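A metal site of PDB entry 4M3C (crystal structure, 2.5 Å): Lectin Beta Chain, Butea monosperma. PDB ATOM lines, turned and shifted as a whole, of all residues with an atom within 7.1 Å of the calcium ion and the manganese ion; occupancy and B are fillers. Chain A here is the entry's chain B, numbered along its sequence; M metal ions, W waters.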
ATOM      1  N   ASP A  88      18.191 -30.762  12.981  1.00  0.00           N
ATOM      2  CA  ASP A  88      18.251 -29.480  12.298  1.00  0.00           C
ATOM      3  C   ASP A  88      19.361 -28.567  12.866  1.00  0.00           C
ATOM      4  O   ASP A  88      20.076 -27.881  12.097  1.00  0.00           O
ATOM      5  CB  ASP A  88      16.891 -28.791  12.378  1.00  0.00           C
ATOM      6  CG  ASP A  88      16.090 -28.910  11.062  1.00  0.00           C
ATOM      7  OD1 ASP A  88      16.577 -28.458   9.999  1.00  0.00           O
ATOM      8  OD2 ASP A  88      14.925 -29.389  11.116  1.00  0.00           O
ATOM      9  N   GLY A  89      19.531 -28.567  14.203  1.00  0.00           N
ATOM     10  CA  GLY A  89      20.632 -27.852  14.814  1.00  0.00           C
ATOM     11  C   GLY A  89      20.344 -27.476  16.250  1.00  0.00           C
ATOM     12  O   GLY A  89      19.266 -27.756  16.768  1.00  0.00           O
ATOM     13  N   ALA A 105      12.082 -27.792  13.764  1.00  0.00           N
ATOM     14  CA  ALA A 105      12.816 -28.062  12.544  1.00  0.00           C
ATOM     15  C   ALA A 105      13.719 -26.826  12.210  1.00  0.00           C
ATOM     16  O   ALA A 105      14.351 -26.282  13.096  1.00  0.00           O
ATOM     17  CB  ALA A 105      11.836 -28.410  11.420  1.00  0.00           C
ATOM     18  N   GLY A 106      13.798 -26.381  10.961  1.00  0.00           N
ATOM     19  CA  GLY A 106      14.777 -25.355  10.584  1.00  0.00           C
ATOM     20  C   GLY A 106      14.677 -24.013  11.288  1.00  0.00           C
ATOM     21  O   GLY A 106      15.570 -23.176  11.183  1.00  0.00           O
ATOM     22  N   PHE A 107      13.588 -23.804  12.009  1.00  0.00           N
ATOM     23  CA  PHE A 107      13.400 -22.592  12.806  1.00  0.00           C
ATOM     24  C   PHE A 107      14.114 -22.691  14.165  1.00  0.00           C
ATOM     25  O   PHE A 107      14.254 -21.693  14.899  1.00  0.00           O
ATOM     26  CB  PHE A 107      11.895 -22.329  13.022  1.00  0.00           C
ATOM     27  CG  PHE A 107      11.105 -22.290  11.738  1.00  0.00           C
ATOM     28  CD1 PHE A 107      10.565 -23.440  11.199  1.00  0.00           C
ATOM     29  CD2 PHE A 107      10.902 -21.088  11.065  1.00  0.00           C
ATOM     30  CE1 PHE A 107       9.846 -23.420  10.031  1.00  0.00           C
ATOM     31  CE2 PHE A 107      10.182 -21.059   9.886  1.00  0.00           C
ATOM     32  CZ  PHE A 107       9.643 -22.226   9.369  1.00  0.00           C
ATOM     33  N   LEU A 108      14.557 -23.896  14.515  1.00  0.00           N
ATOM     34  CA  LEU A 108      15.322 -24.064  15.752  1.00  0.00           C
ATOM     35  C   LEU A 108      14.589 -23.459  16.983  1.00  0.00           C
ATOM     36  O   LEU A 108      15.215 -22.960  17.925  1.00  0.00           O
ATOM     37  CB  LEU A 108      16.718 -23.465  15.562  1.00  0.00           C
ATOM     38  CG  LEU A 108      17.502 -23.904  14.323  1.00  0.00           C
ATOM     39  CD1 LEU A 108      18.943 -23.387  14.325  1.00  0.00           C
ATOM     40  CD2 LEU A 108      17.557 -25.411  14.211  1.00  0.00           C
ATOM     41  N   GLU A 126      23.609 -19.989  15.962  1.00  0.00           N
ATOM     42  CA  GLU A 126      23.185 -21.301  15.567  1.00  0.00           C
ATOM     43  C   GLU A 126      24.347 -22.107  15.040  1.00  0.00           C
ATOM     44  O   GLU A 126      25.278 -21.577  14.377  1.00  0.00           O
ATOM     45  CB  GLU A 126      22.125 -21.228  14.481  1.00  0.00           C
ATOM     46  CG  GLU A 126      22.637 -20.599  13.187  1.00  0.00           C
ATOM     47  CD  GLU A 126      21.674 -20.740  11.999  1.00  0.00           C
ATOM     48  OE1 GLU A 126      20.440 -20.456  12.141  1.00  0.00           O
ATOM     49  OE2 GLU A 126      22.187 -21.128  10.925  1.00  0.00           O
ATOM     50  N   PHE A 127      24.237 -23.401  15.340  1.00  0.00           N
ATOM     51  CA  PHE A 127      25.075 -24.454  14.830  1.00  0.00           C
ATOM     52  C   PHE A 127      24.059 -25.270  14.053  1.00  0.00           C
ATOM     53  O   PHE A 127      23.233 -26.002  14.632  1.00  0.00           O
ATOM     54  CB  PHE A 127      25.676 -25.195  16.008  1.00  0.00           C
ATOM     55  CG  PHE A 127      26.520 -24.313  16.893  1.00  0.00           C
ATOM     56  CD1 PHE A 127      27.890 -24.186  16.677  1.00  0.00           C
ATOM     57  CD2 PHE A 127      25.948 -23.566  17.892  1.00  0.00           C
ATOM     58  CE1 PHE A 127      28.672 -23.355  17.454  1.00  0.00           C
ATOM     59  CE2 PHE A 127      26.729 -22.733  18.689  1.00  0.00           C
ATOM     60  CZ  PHE A 127      28.101 -22.625  18.475  1.00  0.00           C
ATOM     61  N   ASP A 128      24.085 -25.053  12.738  1.00  0.00           N
ATOM     62  CA  ASP A 128      23.017 -25.467  11.820  1.00  0.00           C
ATOM     63  C   ASP A 128      23.448 -26.570  10.858  1.00  0.00           C
ATOM     64  O   ASP A 128      24.383 -26.393  10.046  1.00  0.00           O
ATOM     65  CB  ASP A 128      22.474 -24.263  11.054  1.00  0.00           C
ATOM     66  CG  ASP A 128      21.425 -24.649  10.022  1.00  0.00           C
ATOM     67  OD1 ASP A 128      21.132 -25.843   9.890  1.00  0.00           O
ATOM     68  OD2 ASP A 128      20.897 -23.771   9.315  1.00  0.00           O
ATOM     69  N   THR A 129      22.718 -27.677  10.931  1.00  0.00           N
ATOM     70  CA  THR A 129      23.197 -28.929  10.371  1.00  0.00           C
ATOM     71  C   THR A 129      22.437 -29.425   9.162  1.00  0.00           C
ATOM     72  O   THR A 129      22.628 -30.568   8.760  1.00  0.00           O
ATOM     73  CB  THR A 129      23.171 -30.060  11.421  1.00  0.00           C
ATOM     74  OG1 THR A 129      21.841 -30.163  11.968  1.00  0.00           O
ATOM     75  CG2 THR A 129      24.231 -29.792  12.557  1.00  0.00           C
ATOM     76  N   TYR A 130      21.605 -28.555   8.585  1.00  0.00           N
ATOM     77  CA  TYR A 130      20.731 -28.960   7.482  1.00  0.00           C
ATOM     78  C   TYR A 130      20.244 -27.781   6.620  1.00  0.00           C
ATOM     79  O   TYR A 130      19.638 -26.815   7.118  1.00  0.00           O
ATOM     80  CB  TYR A 130      19.527 -29.719   8.011  1.00  0.00           C
ATOM     81  CG  TYR A 130      18.488 -30.006   6.948  1.00  0.00           C
ATOM     82  CD1 TYR A 130      18.541 -31.196   6.204  1.00  0.00           C
ATOM     83  CD2 TYR A 130      17.464 -29.100   6.672  1.00  0.00           C
ATOM     84  CE1 TYR A 130      17.609 -31.468   5.244  1.00  0.00           C
ATOM     85  CE2 TYR A 130      16.522 -29.376   5.692  1.00  0.00           C
ATOM     86  CZ  TYR A 130      16.605 -30.567   4.989  1.00  0.00           C
ATOM     87  OH  TYR A 130      15.686 -30.869   4.024  1.00  0.00           O
ATOM     88  N   GLU A 131      20.470 -27.904   5.323  1.00  0.00           N
ATOM     89  CA  GLU A 131      20.320 -26.771   4.448  1.00  0.00           C
ATOM     90  C   GLU A 131      18.879 -26.519   4.102  1.00  0.00           C
ATOM     91  O   GLU A 131      18.263 -27.320   3.418  1.00  0.00           O
ATOM     92  CB  GLU A 131      21.134 -26.938   3.168  1.00  0.00           C
ATOM     93  CG  GLU A 131      21.222 -25.620   2.421  1.00  0.00           C
ATOM     94  CD  GLU A 131      21.611 -25.725   0.957  1.00  0.00           C
ATOM     95  OE1 GLU A 131      21.630 -26.820   0.361  1.00  0.00           O
ATOM     96  OE2 GLU A 131      21.906 -24.667   0.389  1.00  0.00           O
ATOM     97  N   ASN A 132      18.346 -25.393   4.595  1.00  0.00           N
ATOM     98  CA  ASN A 132      17.042 -24.913   4.157  1.00  0.00           C
ATOM     99  C   ASN A 132      17.295 -23.828   3.101  1.00  0.00           C
ATOM    100  O   ASN A 132      17.673 -22.706   3.396  1.00  0.00           O
ATOM    101  CB  ASN A 132      16.196 -24.353   5.289  1.00  0.00           C
ATOM    102  CG  ASN A 132      16.093 -25.273   6.482  1.00  0.00           C
ATOM    103  OD1 ASN A 132      15.056 -25.933   6.672  1.00  0.00           O
ATOM    104  ND2 ASN A 132      17.142 -25.294   7.340  1.00  0.00           N
ATOM    105  N   PHE A 135      15.729 -20.388   3.655  1.00  0.00           N
ATOM    106  CA  PHE A 135      16.407 -19.474   4.620  1.00  0.00           C
ATOM    107  C   PHE A 135      17.755 -19.009   4.122  1.00  0.00           C
ATOM    108  O   PHE A 135      18.513 -18.399   4.854  1.00  0.00           O
ATOM    109  CB  PHE A 135      16.574 -20.076   6.017  1.00  0.00           C
ATOM    110  CG  PHE A 135      15.352 -20.766   6.547  1.00  0.00           C
ATOM    111  CD1 PHE A 135      14.070 -20.384   6.122  1.00  0.00           C
ATOM    112  CD2 PHE A 135      15.479 -21.804   7.481  1.00  0.00           C
ATOM    113  CE1 PHE A 135      12.947 -21.051   6.582  1.00  0.00           C
ATOM    114  CE2 PHE A 135      14.357 -22.470   7.951  1.00  0.00           C
ATOM    115  CZ  PHE A 135      13.095 -22.088   7.506  1.00  0.00           C
ATOM    116  N   LEU A 136      18.040 -19.304   2.857  1.00  0.00           N
ATOM    117  CA  LEU A 136      19.344 -19.049   2.261  1.00  0.00           C
ATOM    118  C   LEU A 136      20.505 -19.683   3.054  1.00  0.00           C
ATOM    119  O   LEU A 136      21.610 -19.132   3.070  1.00  0.00           O
ATOM    120  CB  LEU A 136      19.551 -17.552   1.961  1.00  0.00           C
ATOM    121  CG  LEU A 136      18.448 -16.959   1.024  1.00  0.00           C
ATOM    122  CD1 LEU A 136      17.805 -15.670   1.543  1.00  0.00           C
ATOM    123  CD2 LEU A 136      18.853 -16.851  -0.455  1.00  0.00           C
ATOM    124  N   ASP A 137      20.250 -20.840   3.695  1.00  0.00           N
ATOM    125  CA  ASP A 137      21.335 -21.638   4.303  1.00  0.00           C
ATOM    126  C   ASP A 137      22.410 -21.931   3.239  1.00  0.00           C
ATOM    127  O   ASP A 137      22.071 -22.153   2.063  1.00  0.00           O
ATOM    128  CB  ASP A 137      20.830 -22.980   4.896  1.00  0.00           C
ATOM    129  CG  ASP A 137      20.329 -22.859   6.344  1.00  0.00           C
ATOM    130  OD1 ASP A 137      20.584 -21.891   7.066  1.00  0.00           O
ATOM    131  OD2 ASP A 137      19.661 -23.800   6.803  1.00  0.00           O
ATOM    132  N   PRO A 138      23.693 -21.872   3.622  1.00  0.00           N
ATOM    133  CA  PRO A 138      24.783 -22.228   2.697  1.00  0.00           C
ATOM    134  C   PRO A 138      24.842 -23.741   2.455  1.00  0.00           C
ATOM    135  O   PRO A 138      24.325 -24.490   3.269  1.00  0.00           O
ATOM    136  CB  PRO A 138      26.048 -21.726   3.410  1.00  0.00           C
ATOM    137  CG  PRO A 138      25.652 -21.464   4.836  1.00  0.00           C
ATOM    138  CD  PRO A 138      24.172 -21.307   4.903  1.00  0.00           C
ATOM    139  N   ASP A 140      26.659 -26.023   3.104  1.00  0.00           N
ATOM    140  CA  ASP A 140      27.508 -26.768   4.029  1.00  0.00           C
ATOM    141  C   ASP A 140      26.893 -26.605   5.428  1.00  0.00           C
ATOM    142  O   ASP A 140      26.081 -25.716   5.646  1.00  0.00           O
ATOM    143  CB  ASP A 140      29.028 -26.389   3.910  1.00  0.00           C
ATOM    144  CG  ASP A 140      29.324 -24.839   3.879  1.00  0.00           C
ATOM    145  OD1 ASP A 140      29.548 -24.205   4.961  1.00  0.00           O
ATOM    146  OD2 ASP A 140      29.455 -24.262   2.758  1.00  0.00           O
ATOM    147  N   HIS A 142      26.929 -25.206   9.043  1.00  0.00           N
ATOM    148  CA  HIS A 142      27.579 -23.920   9.349  1.00  0.00           C
ATOM    149  C   HIS A 142      27.268 -23.327  10.678  1.00  0.00           C
ATOM    150  O   HIS A 142      26.241 -23.623  11.269  1.00  0.00           O
ATOM    151  CB  HIS A 142      27.145 -22.909   8.316  1.00  0.00           C
ATOM    152  CG  HIS A 142      25.647 -22.810   8.179  1.00  0.00           C
ATOM    153  ND1 HIS A 142      24.937 -23.662   7.416  1.00  0.00           N
ATOM    154  CD2 HIS A 142      24.728 -21.940   8.757  1.00  0.00           C
ATOM    155  CE1 HIS A 142      23.640 -23.340   7.502  1.00  0.00           C
ATOM    156  NE2 HIS A 142      23.520 -22.291   8.320  1.00  0.00           N
ATOM    157  N   ILE A 143      28.142 -22.434  11.129  1.00  0.00           N
ATOM    158  CA  ILE A 143      27.862 -21.546  12.263  1.00  0.00           C
ATOM    159  C   ILE A 143      27.284 -20.258  11.717  1.00  0.00           C
ATOM    160  O   ILE A 143      27.768 -19.708  10.713  1.00  0.00           O
ATOM    161  CB  ILE A 143      29.104 -21.223  13.107  1.00  0.00           C
ATOM    162  CG1 ILE A 143      29.702 -22.508  13.654  1.00  0.00           C
ATOM    163  CG2 ILE A 143      28.726 -20.274  14.251  1.00  0.00           C
ATOM    164  CD1 ILE A 143      31.024 -22.341  14.389  1.00  0.00           C
ATOM    165  N   GLY A 144      26.200 -19.806  12.349  1.00  0.00           N
ATOM    166  CA  GLY A 144      25.450 -18.618  11.888  1.00  0.00           C
ATOM    167  C   GLY A 144      25.075 -17.689  13.034  1.00  0.00           C
ATOM    168  O   GLY A 144      24.798 -18.140  14.156  1.00  0.00           O
ATOM    169  N   ASP A 146      22.178 -15.114  14.034  1.00  0.00           N
ATOM    170  CA  ASP A 146      20.780 -14.782  13.630  1.00  0.00           C
ATOM    171  C   ASP A 146      20.249 -13.663  14.486  1.00  0.00           C
ATOM    172  O   ASP A 146      20.219 -13.739  15.713  1.00  0.00           O
ATOM    173  CB  ASP A 146      19.805 -15.960  13.763  1.00  0.00           C
ATOM    174  CG  ASP A 146      20.352 -17.275  13.203  1.00  0.00           C
ATOM    175  OD1 ASP A 146      21.181 -17.205  12.268  1.00  0.00           O
ATOM    176  OD2 ASP A 146      19.961 -18.360  13.720  1.00  0.00           O
ATOM    177  N   ILE A 150      15.872 -16.323  11.080  1.00  0.00           N
ATOM    178  CA  ILE A 150      16.595 -17.582  10.893  1.00  0.00           C
ATOM    179  C   ILE A 150      17.546 -17.459   9.705  1.00  0.00           C
ATOM    180  O   ILE A 150      18.397 -18.335   9.467  1.00  0.00           O
ATOM    181  CB  ILE A 150      15.617 -18.739  10.620  1.00  0.00           C
ATOM    182  CG1 ILE A 150      16.314 -20.104  10.757  1.00  0.00           C
ATOM    183  CG2 ILE A 150      15.008 -18.582   9.229  1.00  0.00           C
ATOM    184  CD1 ILE A 150      16.808 -20.477  12.139  1.00  0.00           C
ATOM    185  N   LYS A 151      17.399 -16.379   8.967  1.00  0.00           N
ATOM    186  CA  LYS A 151      18.292 -16.047   7.883  1.00  0.00           C
ATOM    187  C   LYS A 151      19.457 -15.260   8.448  1.00  0.00           C
ATOM    188  O   LYS A 151      19.366 -14.068   8.657  1.00  0.00           O
ATOM    189  CB  LYS A 151      17.521 -15.250   6.813  1.00  0.00           C
ATOM    190  CG  LYS A 151      18.206 -15.238   5.457  1.00  0.00           C
ATOM    191  CD  LYS A 151      19.003 -13.967   5.175  1.00  0.00           C
ATOM    192  CE  LYS A 151      18.994 -13.665   3.668  1.00  0.00           C
ATOM    193  NZ  LYS A 151      20.333 -13.288   3.119  1.00  0.00           N
ATOM    194  N   SER A 152      20.567 -15.947   8.691  1.00  0.00           N
ATOM    195  CA  SER A 152      21.714 -15.379   9.382  1.00  0.00           C
ATOM    196  C   SER A 152      22.294 -14.150   8.705  1.00  0.00           C
ATOM    197  O   SER A 152      22.433 -14.150   7.501  1.00  0.00           O
ATOM    198  CB  SER A 152      22.775 -16.477   9.461  1.00  0.00           C
ATOM    199  OG  SER A 152      22.216 -17.673   9.974  1.00  0.00           O
ATOM    200  N   THR A 155      27.588 -16.152   8.291  1.00  0.00           N
ATOM    201  CA  THR A 155      27.857 -17.568   8.488  1.00  0.00           C
ATOM    202  C   THR A 155      29.304 -18.003   8.160  1.00  0.00           C
ATOM    203  O   THR A 155      29.982 -17.346   7.362  1.00  0.00           O
ATOM    204  CB  THR A 155      26.910 -18.447   7.640  1.00  0.00           C
ATOM    205  OG1 THR A 155      27.209 -18.226   6.265  1.00  0.00           O
ATOM    206  CG2 THR A 155      25.456 -18.105   7.868  1.00  0.00           C
HETATM  207 CA    CA M   1      19.030 -25.098   8.707  1.00  0.00          CA
HETATM  208 MN    MN M   2      21.463 -21.721   9.063  1.00  0.00          MN
HETATM  209  O   HOH W   1      17.918 -23.412   9.252  1.00  0.00           O
HETATM  210  O   HOH W   2      21.943 -19.500   8.215  1.00  0.00           O
HETATM  211  O   HOH W   3      18.383 -26.544   9.911  1.00  0.00           O
HETATM  212  O   HOH W   4      19.379 -20.853   9.529  1.00  0.00           O
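The backbone NH (N) of Glu 126 lies within hydrogen-bond range of the backbone carbonyl oxygen (O) of Gly 144 (2.8 Å). The side-chain carboxylate of Glu 126 sits close to the side-chain carboxylate of Asp 146 (2.7 Å). ND1 of His 142 is in hydrogen-bond range of O of Asp 140.
Within 4 Å of the calcium ion: Asp 128, Tyr 130, Asn 132 and Asp 137.
The nearest printed residue that does not touch the manganese ion is Ser 152 (4.2 Å).
The calcium ion is bound by water W3 (2.0 Å). Water W1 is bound to the calcium ion, at 2.1 Å. ND2 of Asn 132 binds the calcium ion. OD2 of Asp 128 binds the calcium ion (2.4 Å). OD2 of Asp 137 is bound to the calcium ion. O of Tyr 130 is bound to the calcium ion (2.4 Å). OD1 of Asp 128 is bound to the calcium ion (2.5 Å).
The manganese ion is bound by OE2 of Glu 126 (2.1 Å), OD2 of Asp 128 (2.1 Å), OD1 of Asp 137 (2.2 Å), NE2 of His 142 (2.3 Å), water W4 (2.3 Å) and water W2 (2.4 Å).
Water W4 lies within hydrogen-bond range of O of Ile 150 (2.7 Å) and OE1 of Glu 126 (2.8 Å).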
